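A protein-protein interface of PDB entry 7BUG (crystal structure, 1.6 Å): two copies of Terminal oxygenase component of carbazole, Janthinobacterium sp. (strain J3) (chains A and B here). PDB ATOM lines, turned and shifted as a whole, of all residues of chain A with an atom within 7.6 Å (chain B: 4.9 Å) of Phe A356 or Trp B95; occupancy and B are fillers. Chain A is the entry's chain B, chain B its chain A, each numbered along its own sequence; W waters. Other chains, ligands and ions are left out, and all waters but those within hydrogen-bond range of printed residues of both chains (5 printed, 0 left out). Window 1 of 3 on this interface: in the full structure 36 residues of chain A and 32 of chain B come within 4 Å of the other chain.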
ATOM      1  N   ASP A 180       9.136  10.166   5.479  1.00  0.00           N
ATOM      2  CA  ASP A 180       9.808  11.176   6.306  1.00  0.00           C
ATOM      3  C   ASP A 180       9.860  12.512   5.580  1.00  0.00           C
ATOM      4  O   ASP A 180      10.537  12.631   4.562  1.00  0.00           O
ATOM      5  CB  ASP A 180      11.195  10.639   6.532  1.00  0.00           C
ATOM      6  CG  ASP A 180      12.027  11.437   7.460  1.00  0.00           C
ATOM      7  OD1 ASP A 180      11.889  12.687   7.463  1.00  0.00           O
ATOM      8  OD2 ASP A 180      12.871  10.764   8.106  1.00  0.00           O
ATOM      9  N   PRO A 181       9.169  13.566   6.034  1.00  0.00           N
ATOM     10  CA  PRO A 181       9.148  14.795   5.268  1.00  0.00           C
ATOM     11  C   PRO A 181      10.518  15.478   5.149  1.00  0.00           C
ATOM     12  O   PRO A 181      10.743  16.194   4.206  1.00  0.00           O
ATOM     13  CB  PRO A 181       8.175  15.674   6.092  1.00  0.00           C
ATOM     14  CG  PRO A 181       7.334  14.667   6.854  1.00  0.00           C
ATOM     15  CD  PRO A 181       8.307  13.594   7.229  1.00  0.00           C
ATOM     16  N   SER A 182      11.383  15.299   6.131  1.00  0.00           N
ATOM     17  CA  SER A 182      12.645  16.055   6.185  1.00  0.00           C
ATOM     18  C   SER A 182      13.782  15.288   5.513  1.00  0.00           C
ATOM     19  O   SER A 182      14.850  15.874   5.276  1.00  0.00           O
ATOM     20  CB  SER A 182      13.000  16.448   7.610  1.00  0.00           C
ATOM     21  OG  SER A 182      12.154  17.510   7.992  1.00  0.00           O
ATOM     22  N   HIS A 183      13.557  14.007   5.182  1.00  0.00           N
ATOM     23  CA  HIS A 183      14.661  13.207   4.616  1.00  0.00           C
ATOM     24  C   HIS A 183      15.025  13.700   3.223  1.00  0.00           C
ATOM     25  O   HIS A 183      16.094  13.305   2.757  1.00  0.00           O
ATOM     26  CB  HIS A 183      14.337  11.712   4.568  1.00  0.00           C
ATOM     27  CG  HIS A 183      13.737  11.240   3.317  1.00  0.00           C
ATOM     28  ND1 HIS A 183      12.401  11.396   2.995  1.00  0.00           N
ATOM     29  CD2 HIS A 183      14.319  10.685   2.225  1.00  0.00           C
ATOM     30  CE1 HIS A 183      12.181  10.935   1.783  1.00  0.00           C
ATOM     31  NE2 HIS A 183      13.326  10.462   1.305  1.00  0.00           N
ATOM     32  N   TYR A 185      16.385  16.127   2.278  1.00  0.00           N
ATOM     33  CA  TYR A 185      17.780  16.635   2.348  1.00  0.00           C
ATOM     34  C   TYR A 185      18.746  15.679   1.637  1.00  0.00           C
ATOM     35  O   TYR A 185      19.697  16.149   0.992  1.00  0.00           O
ATOM     36  CB  TYR A 185      18.144  16.881   3.788  1.00  0.00           C
ATOM     37  CG  TYR A 185      19.477  17.523   3.959  1.00  0.00           C
ATOM     38  CD1 TYR A 185      19.638  18.873   3.725  1.00  0.00           C
ATOM     39  CD2 TYR A 185      20.588  16.777   4.295  1.00  0.00           C
ATOM     40  CE1 TYR A 185      20.892  19.481   3.809  1.00  0.00           C
ATOM     41  CE2 TYR A 185      21.834  17.370   4.403  1.00  0.00           C
ATOM     42  CZ  TYR A 185      21.979  18.723   4.160  1.00  0.00           C
ATOM     43  OH  TYR A 185      23.229  19.311   4.225  1.00  0.00           O
ATOM     44  N   PHE A 204      11.265  21.671   5.454  1.00  0.00           N
ATOM     45  CA  PHE A 204      10.109  22.554   5.728  1.00  0.00           C
ATOM     46  C   PHE A 204      10.126  22.989   7.194  1.00  0.00           C
ATOM     47  O   PHE A 204      10.340  22.191   8.114  1.00  0.00           O
ATOM     48  CB  PHE A 204       8.789  21.880   5.382  1.00  0.00           C
ATOM     49  CG  PHE A 204       8.616  21.517   3.938  1.00  0.00           C
ATOM     50  CD1 PHE A 204       8.066  22.416   3.033  1.00  0.00           C
ATOM     51  CD2 PHE A 204       9.031  20.272   3.487  1.00  0.00           C
ATOM     52  CE1 PHE A 204       7.958  22.082   1.688  1.00  0.00           C
ATOM     53  CE2 PHE A 204       8.892  19.941   2.151  1.00  0.00           C
ATOM     54  CZ  PHE A 204       8.373  20.839   1.259  1.00  0.00           C
ATOM     55  N   PRO A 206       7.562  23.839   9.917  1.00  0.00           N
ATOM     56  CA  PRO A 206       6.123  23.574   9.964  1.00  0.00           C
ATOM     57  C   PRO A 206       5.353  24.902  10.044  1.00  0.00           C
ATOM     58  O   PRO A 206       5.900  25.862  10.595  1.00  0.00           O
ATOM     59  CB  PRO A 206       5.958  22.692  11.192  1.00  0.00           C
ATOM     60  CG  PRO A 206       7.321  22.032  11.292  1.00  0.00           C
ATOM     61  CD  PRO A 206       8.283  23.163  10.998  1.00  0.00           C
ATOM     62  N   GLU A 353      15.852   7.140  20.180  1.00  0.00           N
ATOM     63  CA  GLU A 353      15.715   8.185  19.143  1.00  0.00           C
ATOM     64  C   GLU A 353      15.222   9.499  19.763  1.00  0.00           C
ATOM     65  O   GLU A 353      14.448   9.484  20.784  1.00  0.00           O
ATOM     66  CB  GLU A 353      14.768   7.726  18.043  1.00  0.00           C
ATOM     67  CG  GLU A 353      13.338   7.572  18.479  1.00  0.00           C
ATOM     68  CD  GLU A 353      12.314   6.990  17.532  1.00  0.00           C
ATOM     69  OE1 GLU A 353      12.686   6.386  16.481  1.00  0.00           O
ATOM     70  OE2 GLU A 353      11.074   7.144  17.870  1.00  0.00           O
ATOM     71  N   ILE A 354      15.652  10.605  19.214  1.00  0.00           N
ATOM     72  CA  ILE A 354      15.101  11.932  19.575  1.00  0.00           C
ATOM     73  C   ILE A 354      14.450  12.529  18.345  1.00  0.00           C
ATOM     74  O   ILE A 354      15.138  12.959  17.382  1.00  0.00           O
ATOM     75  CB  ILE A 354      16.191  12.826  20.161  1.00  0.00           C
ATOM     76  CG1 ILE A 354      16.880  12.156  21.362  1.00  0.00           C
ATOM     77  CG2 ILE A 354      15.550  14.195  20.466  1.00  0.00           C
ATOM     78  CD1 ILE A 354      18.041  12.923  21.888  1.00  0.00           C
ATOM     79  N   LEU A 355      13.140  12.547  18.338  1.00  0.00           N
ATOM     80  CA  LEU A 355      12.376  13.020  17.177  1.00  0.00           C
ATOM     81  C   LEU A 355      12.261  14.540  17.191  1.00  0.00           C
ATOM     82  O   LEU A 355      12.403  15.148  18.245  1.00  0.00           O
ATOM     83  CB  LEU A 355      10.995  12.379  17.211  1.00  0.00           C
ATOM     84  CG  LEU A 355      11.016  10.848  17.118  1.00  0.00           C
ATOM     85  CD1 LEU A 355       9.611  10.311  16.935  1.00  0.00           C
ATOM     86  CD2 LEU A 355      11.924  10.329  16.004  1.00  0.00           C
ATOM     87  N   PHE A 356      12.020  15.110  16.020  1.00  0.00           N
ATOM     88  CA  PHE A 356      11.686  16.548  15.883  1.00  0.00           C
ATOM     89  C   PHE A 356      10.398  16.708  15.090  1.00  0.00           C
ATOM     90  O   PHE A 356       9.683  15.762  14.852  1.00  0.00           O
ATOM     91  CB  PHE A 356      12.889  17.367  15.432  1.00  0.00           C
ATOM     92  CG  PHE A 356      13.241  17.373  13.965  1.00  0.00           C
ATOM     93  CD1 PHE A 356      13.078  16.223  13.196  1.00  0.00           C
ATOM     94  CD2 PHE A 356      13.809  18.478  13.365  1.00  0.00           C
ATOM     95  CE1 PHE A 356      13.468  16.174  11.861  1.00  0.00           C
ATOM     96  CE2 PHE A 356      14.201  18.427  12.039  1.00  0.00           C
ATOM     97  CZ  PHE A 356      14.047  17.279  11.284  1.00  0.00           C
ATOM     98  N   GLU A 357      10.054  17.970  14.803  1.00  0.00           N
ATOM     99  CA  GLU A 357       8.672  18.311  14.452  1.00  0.00           C
ATOM    100  C   GLU A 357       8.163  17.531  13.234  1.00  0.00           C
ATOM    101  O   GLU A 357       7.002  17.039  13.276  1.00  0.00           O
ATOM    102  CB  GLU A 357       8.585  19.822  14.256  1.00  0.00           C
ATOM    103  CG  GLU A 357       8.695  20.584  15.545  1.00  0.00           C
ATOM    104  CD  GLU A 357      10.076  20.915  16.077  1.00  0.00           C
ATOM    105  OE1 GLU A 357      11.065  20.452  15.468  1.00  0.00           O
ATOM    106  OE2 GLU A 357      10.171  21.728  17.049  1.00  0.00           O
ATOM    107  N   SER A 358       8.935  17.465  12.139  1.00  0.00           N
ATOM    108  CA  SER A 358       8.497  16.782  10.907  1.00  0.00           C
ATOM    109  C   SER A 358       8.264  15.297  11.158  1.00  0.00           C
ATOM    110  O   SER A 358       7.527  14.696  10.406  1.00  0.00           O
ATOM    111  CB  SER A 358       9.448  17.000   9.760  1.00  0.00           C
ATOM    112  OG  SER A 358      10.712  16.490  10.069  1.00  0.00           O
ATOM    113  N   ASP A 359       8.762  14.756  12.249  1.00  0.00           N
ATOM    114  CA  ASP A 359       8.523  13.347  12.600  1.00  0.00           C
ATOM    115  C   ASP A 359       7.089  13.124  13.080  1.00  0.00           C
ATOM    116  O   ASP A 359       6.700  11.948  13.251  1.00  0.00           O
ATOM    117  CB  ASP A 359       9.518  12.835  13.628  1.00  0.00           C
ATOM    118  CG  ASP A 359      10.942  12.806  13.105  1.00  0.00           C
ATOM    119  OD1 ASP A 359      11.125  12.441  11.901  1.00  0.00           O
ATOM    120  OD2 ASP A 359      11.850  13.109  13.903  1.00  0.00           O
ATOM    121  N   GLU A 360       6.291  14.182  13.217  1.00  0.00           N
ATOM    122  CA  GLU A 360       4.835  13.997  13.480  1.00  0.00           C
ATOM    123  C   GLU A 360       4.236  13.065  12.421  1.00  0.00           C
ATOM    124  O   GLU A 360       3.391  12.252  12.768  1.00  0.00           O
ATOM    125  CB  GLU A 360       4.122  15.365  13.482  1.00  0.00           C
ATOM    126  CG  GLU A 360       2.606  15.252  13.607  1.00  0.00           C
ATOM    127  CD  GLU A 360       1.895  16.609  13.735  1.00  0.00           C
ATOM    128  OE1 GLU A 360       0.662  16.693  13.467  1.00  0.00           O
ATOM    129  OE2 GLU A 360       2.572  17.597  14.085  1.00  0.00           O
ATOM    130  N   ALA A 361       4.664  13.166  11.147  1.00  0.00           N
ATOM    131  CA  ALA A 361       4.204  12.298  10.048  1.00  0.00           C
ATOM    132  C   ALA A 361       4.515  10.835  10.373  1.00  0.00           C
ATOM    133  O   ALA A 361       3.630   9.936  10.161  1.00  0.00           O
ATOM    134  CB  ALA A 361       4.817  12.708   8.718  1.00  0.00           C
ATOM    135  N   VAL A 363       5.245   9.465  13.363  1.00  0.00           N
ATOM    136  CA  VAL A 363       4.511   8.985  14.563  1.00  0.00           C
ATOM    137  C   VAL A 363       3.045   8.723  14.160  1.00  0.00           C
ATOM    138  O   VAL A 363       2.447   7.713  14.675  1.00  0.00           O
ATOM    139  CB  VAL A 363       4.604   9.999  15.703  1.00  0.00           C
ATOM    140  CG1 VAL A 363       3.626   9.690  16.822  1.00  0.00           C
ATOM    141  CG2 VAL A 363       6.007  10.081  16.248  1.00  0.00           C
ATOM    142  N   CYS B  69      24.248  10.098  15.295  1.00  0.00           N
ATOM    143  CA  CYS B  69      23.306  11.228  15.321  1.00  0.00           C
ATOM    144  C   CYS B  69      22.281  11.047  16.464  1.00  0.00           C
ATOM    145  O   CYS B  69      21.766   9.943  16.654  1.00  0.00           O
ATOM    146  CB  CYS B  69      22.638  11.398  13.973  1.00  0.00           C
ATOM    147  SG  CYS B  69      21.680  12.930  13.887  1.00  0.00           S
ATOM    148  N   LEU B  70      21.941  12.128  17.157  1.00  0.00           N
ATOM    149  CA  LEU B  70      20.893  12.115  18.220  1.00  0.00           C
ATOM    150  C   LEU B  70      19.516  11.771  17.668  1.00  0.00           C
ATOM    151  O   LEU B  70      18.649  11.330  18.421  1.00  0.00           O
ATOM    152  CB  LEU B  70      20.835  13.495  18.862  1.00  0.00           C
ATOM    153  CG  LEU B  70      22.046  13.903  19.663  1.00  0.00           C
ATOM    154  CD1 LEU B  70      21.819  15.285  20.292  1.00  0.00           C
ATOM    155  CD2 LEU B  70      22.467  12.879  20.693  1.00  0.00           C
ATOM    156  N   HIS B  71      19.260  12.046  16.398  1.00  0.00           N
ATOM    157  CA  HIS B  71      17.911  11.969  15.806  1.00  0.00           C
ATOM    158  C   HIS B  71      17.535  10.489  15.552  1.00  0.00           C
ATOM    159  O   HIS B  71      16.736   9.914  16.304  1.00  0.00           O
ATOM    160  CB  HIS B  71      17.906  12.864  14.555  1.00  0.00           C
ATOM    161  CG  HIS B  71      16.632  12.854  13.833  1.00  0.00           C
ATOM    162  ND1 HIS B  71      16.609  12.908  12.452  1.00  0.00           N
ATOM    163  CD2 HIS B  71      15.360  12.793  14.276  1.00  0.00           C
ATOM    164  CE1 HIS B  71      15.347  12.906  12.052  1.00  0.00           C
ATOM    165  NE2 HIS B  71      14.539  12.854  13.200  1.00  0.00           N
ATOM    166  N   ILE B  88      29.683  19.993  12.098  1.00  0.00           N
ATOM    167  CA  ILE B  88      29.385  18.880  11.157  1.00  0.00           C
ATOM    168  C   ILE B  88      27.870  18.785  11.051  1.00  0.00           C
ATOM    169  O   ILE B  88      27.189  18.958  12.098  1.00  0.00           O
ATOM    170  CB  ILE B  88      30.046  17.535  11.579  1.00  0.00           C
ATOM    171  CG1 ILE B  88      29.760  16.414  10.567  1.00  0.00           C
ATOM    172  CG2 ILE B  88      29.681  17.170  12.994  1.00  0.00           C
ATOM    173  CD1 ILE B  88      30.640  15.165  10.735  1.00  0.00           C
ATOM    174  N   THR B  89      27.366  18.492   9.852  1.00  0.00           N
ATOM    175  CA  THR B  89      25.931  18.404   9.557  1.00  0.00           C
ATOM    176  C   THR B  89      25.641  16.930   9.251  1.00  0.00           C
ATOM    177  O   THR B  89      26.260  16.390   8.292  1.00  0.00           O
ATOM    178  CB  THR B  89      25.585  19.322   8.366  1.00  0.00           C
ATOM    179  OG1 THR B  89      25.828  20.661   8.806  1.00  0.00           O
ATOM    180  CG2 THR B  89      24.173  19.144   7.879  1.00  0.00           C
ATOM    181  N   CYS B  90      24.732  16.326   9.979  1.00  0.00           N
ATOM    182  CA  CYS B  90      24.305  14.945   9.637  1.00  0.00           C
ATOM    183  C   CYS B  90      23.771  14.964   8.211  1.00  0.00           C
ATOM    184  O   CYS B  90      22.998  15.875   7.820  1.00  0.00           O
ATOM    185  CB  CYS B  90      23.269  14.456  10.625  1.00  0.00           C
ATOM    186  SG  CYS B  90      22.761  12.765  10.250  1.00  0.00           S
ATOM    187  N   HIS B  93      19.053  14.412   7.983  1.00  0.00           N
ATOM    188  CA  HIS B  93      18.086  15.524   8.147  1.00  0.00           C
ATOM    189  C   HIS B  93      18.825  16.786   8.556  1.00  0.00           C
ATOM    190  O   HIS B  93      18.192  17.692   9.022  1.00  0.00           O
ATOM    191  CB  HIS B  93      16.940  15.208   9.107  1.00  0.00           C
ATOM    192  CG  HIS B  93      16.396  13.836   8.946  1.00  0.00           C
ATOM    193  ND1 HIS B  93      16.978  12.726   9.542  1.00  0.00           N
ATOM    194  CD2 HIS B  93      15.286  13.405   8.307  1.00  0.00           C
ATOM    195  CE1 HIS B  93      16.268  11.657   9.195  1.00  0.00           C
ATOM    196  NE2 HIS B  93      15.214  12.045   8.448  1.00  0.00           N
ATOM    197  N   ALA B  94      20.130  16.801   8.418  1.00  0.00           N
ATOM    198  CA  ALA B  94      20.938  18.031   8.570  1.00  0.00           C
ATOM    199  C   ALA B  94      20.897  18.612   9.984  1.00  0.00           C
ATOM    200  O   ALA B  94      21.188  19.844  10.142  1.00  0.00           O
ATOM    201  CB  ALA B  94      20.543  19.079   7.552  1.00  0.00           C
ATOM    202  N   TRP B  95      20.714  17.789  11.014  1.00  0.00           N
ATOM    203  CA  TRP B  95      21.064  18.218  12.382  1.00  0.00           C
ATOM    204  C   TRP B  95      22.544  18.556  12.412  1.00  0.00           C
ATOM    205  O   TRP B  95      23.412  17.792  11.988  1.00  0.00           O
ATOM    206  CB  TRP B  95      20.719  17.172  13.438  1.00  0.00           C
ATOM    207  CG  TRP B  95      19.267  16.938  13.638  1.00  0.00           C
ATOM    208  CD1 TRP B  95      18.248  17.003  12.733  1.00  0.00           C
ATOM    209  CD2 TRP B  95      18.687  16.535  14.880  1.00  0.00           C
ATOM    210  NE1 TRP B  95      17.058  16.695  13.341  1.00  0.00           N
ATOM    211  CE2 TRP B  95      17.305  16.383  14.647  1.00  0.00           C
ATOM    212  CE3 TRP B  95      19.221  16.243  16.137  1.00  0.00           C
ATOM    213  CZ2 TRP B  95      16.444  15.944  15.655  1.00  0.00           C
ATOM    214  CZ3 TRP B  95      18.346  15.857  17.143  1.00  0.00           C
ATOM    215  CH2 TRP B  95      16.984  15.718  16.888  1.00  0.00           C
ATOM    216  N   THR B  96      22.888  19.757  12.889  1.00  0.00           N
ATOM    217  CA  THR B  96      24.246  20.301  12.828  1.00  0.00           C
ATOM    218  C   THR B  96      24.793  20.508  14.241  1.00  0.00           C
ATOM    219  O   THR B  96      24.125  21.179  15.074  1.00  0.00           O
ATOM    220  CB  THR B  96      24.217  21.614  12.048  1.00  0.00           C
ATOM    221  OG1 THR B  96      23.763  21.293  10.726  1.00  0.00           O
ATOM    222  CG2 THR B  96      25.584  22.260  11.986  1.00  0.00           C
ATOM    223  N   TYR B  97      25.997  19.992  14.473  1.00  0.00           N
ATOM    224  CA  TYR B  97      26.641  19.951  15.798  1.00  0.00           C
ATOM    225  C   TYR B  97      27.956  20.727  15.772  1.00  0.00           C
ATOM    226  O   TYR B  97      28.712  20.683  14.812  1.00  0.00           O
ATOM    227  CB  TYR B  97      26.900  18.508  16.200  1.00  0.00           C
ATOM    228  CG  TYR B  97      25.668  17.633  16.135  1.00  0.00           C
ATOM    229  CD1 TYR B  97      24.841  17.512  17.242  1.00  0.00           C
ATOM    230  CD2 TYR B  97      25.412  16.839  15.034  1.00  0.00           C
ATOM    231  CE1 TYR B  97      23.756  16.664  17.239  1.00  0.00           C
ATOM    232  CE2 TYR B  97      24.313  15.999  15.002  1.00  0.00           C
ATOM    233  CZ  TYR B  97      23.490  15.902  16.115  1.00  0.00           C
ATOM    234  OH  TYR B  97      22.467  14.983  16.060  1.00  0.00           O
ATOM    235  N   LEU B 104      23.836  20.888  19.536  1.00  0.00           N
ATOM    236  CA  LEU B 104      22.969  20.977  18.344  1.00  0.00           C
ATOM    237  C   LEU B 104      22.697  22.462  18.097  1.00  0.00           C
ATOM    238  O   LEU B 104      21.821  23.022  18.791  1.00  0.00           O
ATOM    239  CB  LEU B 104      21.691  20.197  18.589  1.00  0.00           C
ATOM    240  CG  LEU B 104      20.707  20.143  17.442  1.00  0.00           C
ATOM    241  CD1 LEU B 104      21.265  19.527  16.164  1.00  0.00           C
ATOM    242  CD2 LEU B 104      19.443  19.435  17.883  1.00  0.00           C
ATOM    243  N   ASP B 106      22.054  24.046  14.919  1.00  0.00           N
ATOM    244  CA  ASP B 106      21.270  24.390  13.708  1.00  0.00           C
ATOM    245  C   ASP B 106      20.641  23.079  13.224  1.00  0.00           C
ATOM    246  O   ASP B 106      21.215  22.007  13.455  1.00  0.00           O
ATOM    247  CB  ASP B 106      22.127  25.034  12.625  1.00  0.00           C
ATOM    248  CG  ASP B 106      22.418  26.504  12.872  1.00  0.00           C
ATOM    249  OD1 ASP B 106      21.450  27.313  12.754  1.00  0.00           O
ATOM    250  OD2 ASP B 106      23.618  26.838  13.169  1.00  0.00           O
ATOM    251  N   ILE B 107      19.524  23.194  12.541  1.00  0.00           N
ATOM    252  CA  ILE B 107      18.987  22.049  11.752  1.00  0.00           C
ATOM    253  C   ILE B 107      18.566  22.559  10.382  1.00  0.00           C
ATOM    254  O   ILE B 107      17.594  23.349  10.321  1.00  0.00           O
ATOM    255  CB  ILE B 107      17.822  21.331  12.446  1.00  0.00           C
ATOM    256  CG1 ILE B 107      18.165  20.861  13.856  1.00  0.00           C
ATOM    257  CG2 ILE B 107      17.335  20.164  11.562  1.00  0.00           C
ATOM    258  CD1 ILE B 107      17.015  20.315  14.631  1.00  0.00           C
ATOM    259  N   THR B 109      17.046  21.376   7.811  1.00  0.00           N
ATOM    260  CA  THR B 109      15.700  20.993   7.354  1.00  0.00           C
ATOM    261  C   THR B 109      14.588  21.651   8.158  1.00  0.00           C
ATOM    262  O   THR B 109      13.438  21.538   7.721  1.00  0.00           O
ATOM    263  CB  THR B 109      15.561  19.468   7.427  1.00  0.00           C
ATOM    264  OG1 THR B 109      15.805  19.009   8.774  1.00  0.00           O
ATOM    265  CG2 THR B 109      16.469  18.817   6.410  1.00  0.00           C
ATOM    266  N   ASN B 110      14.885  22.299   9.272  1.00  0.00           N
ATOM    267  CA  ASN B 110      13.856  22.982  10.087  1.00  0.00           C
ATOM    268  C   ASN B 110      14.529  23.980  11.012  1.00  0.00           C
ATOM    269  O   ASN B 110      14.864  23.699  12.153  1.00  0.00           O
ATOM    270  CB  ASN B 110      12.965  22.038  10.875  1.00  0.00           C
ATOM    271  CG  ASN B 110      11.916  22.831  11.639  1.00  0.00           C
ATOM    272  OD1 ASN B 110      11.871  24.062  11.476  1.00  0.00           O
ATOM    273  ND2 ASN B 110      11.176  22.168  12.548  1.00  0.00           N
ATOM    274  N   SER B 113      13.096  24.526  14.604  1.00  0.00           N
ATOM    275  CA  SER B 113      12.921  23.417  15.553  1.00  0.00           C
ATOM    276  C   SER B 113      13.164  23.845  16.993  1.00  0.00           C
ATOM    277  O   SER B 113      14.238  24.426  17.279  1.00  0.00           O
ATOM    278  CB  SER B 113      13.853  22.278  15.221  1.00  0.00           C
ATOM    279  OG  SER B 113      13.588  21.147  16.047  1.00  0.00           O
ATOM    280  N   GLN B 115      14.248  21.725  19.019  1.00  0.00           N
ATOM    281  CA  GLN B 115      15.443  20.952  19.467  1.00  0.00           C
ATOM    282  C   GLN B 115      16.728  21.812  19.446  1.00  0.00           C
ATOM    283  O   GLN B 115      17.680  21.469  20.162  1.00  0.00           O
ATOM    284  CB  GLN B 115      15.611  19.685  18.625  1.00  0.00           C
ATOM    285  CG  GLN B 115      14.498  18.664  18.702  1.00  0.00           C
ATOM    286  CD  GLN B 115      14.359  18.009  20.061  1.00  0.00           C
ATOM    287  OE1 GLN B 115      15.062  18.337  21.009  1.00  0.00           O
ATOM    288  NE2 GLN B 115      13.453  17.052  20.166  1.00  0.00           N
HETATM  289  O   HOH W   1       9.382  23.670  14.266  1.00  0.00           O
HETATM  290  O   HOH W   2      11.014  19.835   8.996  1.00  0.00           O
HETATM  291  O   HOH W   3      13.013  10.730  10.945  1.00  0.00           O
HETATM  292  O   HOH W   4      11.159  19.283  11.702  1.00  0.00           O
HETATM  293  O   HOH W   5      11.712  14.297  20.821  1.00  0.00           O
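The side-chain sulfur (SG) of Cys B69 lies close to the backbone NH (N) of His B71, at 3.6 Å. The side-chain hydroxyl of Ser A182 lies within hydrogen-bond range of the side-chain hydroxyl of Ser A358. O of Ala B94 is in hydrogen-bond range of OG1 of Thr B96 (3.0 Å). OD1 of Asp A180 sits at hydrogen-bond distance from N of Ser A182, 3.0 Å away. The side-chain hydroxyl of Ser B113 sits at hydrogen-bond distance from the backbone NH of Gln B115, 3.1 Å away. O of Asp A180 is in hydrogen-bond range of ND1 of His A183, 2.7 Å away.
Hydrophobic or aromatic side chains of chain A that line the printed part of chain B: His A183, Tyr A185, Pro A206, Ile A354 and Phe A356.
A ring nitrogen (NE2) of His B71 is in hydrogen-bond range of the side-chain carboxylate (OD2) of Asp A359 (2.8 Å). The side-chain carboxylate (OD2) of Asp A180 lies within hydrogen-bond range of a ring nitrogen (NE2) of His B93. The backbone carbonyl oxygen (O) of His B71 sits at hydrogen-bond distance from the backbone NH (N) of Ile A354, at 3.2 Å. The backbone carbonyl oxygen (O) of Leu A355 lies within hydrogen-bond range of the side-chain amide nitrogen (NE2) of Gln B115 (2.9 Å). The side-chain carboxylate (OE1) of Glu A357 sits at hydrogen-bond distance from the side-chain hydroxyl (OG) of Ser B113, at 2.7 Å. ND2 of Asn B110 is in hydrogen-bond range of OE1 of Glu A357 (3.4 Å). O of Thr B109 lies within hydrogen-bond range of N of Phe A204 (3.1 Å). N of Ile A354 sits at hydrogen-bond distance from O of Leu B70 (3.2 Å).
Water W2 lies within hydrogen-bond range of the backbone carbonyl oxygen (O) of Phe A204 (2.6 Å), the side-chain hydroxyl (OG) of Ser A182 (2.8 Å) and the backbone carbonyl oxygen (O) of Thr B109 (3.2 Å). Water W3 lies within hydrogen-bond range of OD1 of Asp A359 (2.7 Å), OD2 of Asp A180 (2.8 Å) and NE2 of His B71 (3.5 Å). Water W5 lies within hydrogen-bond range of O of Leu A355 and NE2 of Gln B115. Water W1 lies within hydrogen-bond range of ND2 of Asn B110 (2.9 Å) and OE2 of Glu A357 (3.5 Å). Water W4 lies within hydrogen-bond range of the backbone NH of Ser A358 and the side-chain amide nitrogen of Asn B110.
Of the printed residues of chain B, Phe A356 touches His B71, Trp B95, Ile B107, Thr B109, Asn B110, Ser B113 and Gln B115. Of the printed residues of chain B, Glu A353 touches His B71. Printed residues of chain A within 4 Å of Ser B113: Phe A356 and Glu A357. Pro A181 touches none of the printed residues of chain B. Glu A360 touches none of the printed residues of chain B. The nearest printed residue of chain B that does not touch Phe A356 is His B93 (4.2 Å).
C of Ser A182 touches CD2 of His B93, at 3.7 Å. Cys B90 touches Tyr A185 (O to CE2, 3.9 Å). Tyr A185 touches Ala B94. Pro A206 touches Asn B110. Glu A353 touches His B71 (CB to O, 3.4 Å). CG2 of Ile A354 touches NE2 of Gln B115, at 3.6 Å. NE1 of Trp B95 touches CE2 of Phe A356, at 3.6 Å. Ile B107 touches Phe A356. Phe A356 touches Thr B109. CB of Phe A356 touches CG of Gln B115, 3.9 Å away.
No position is printed for both chains.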
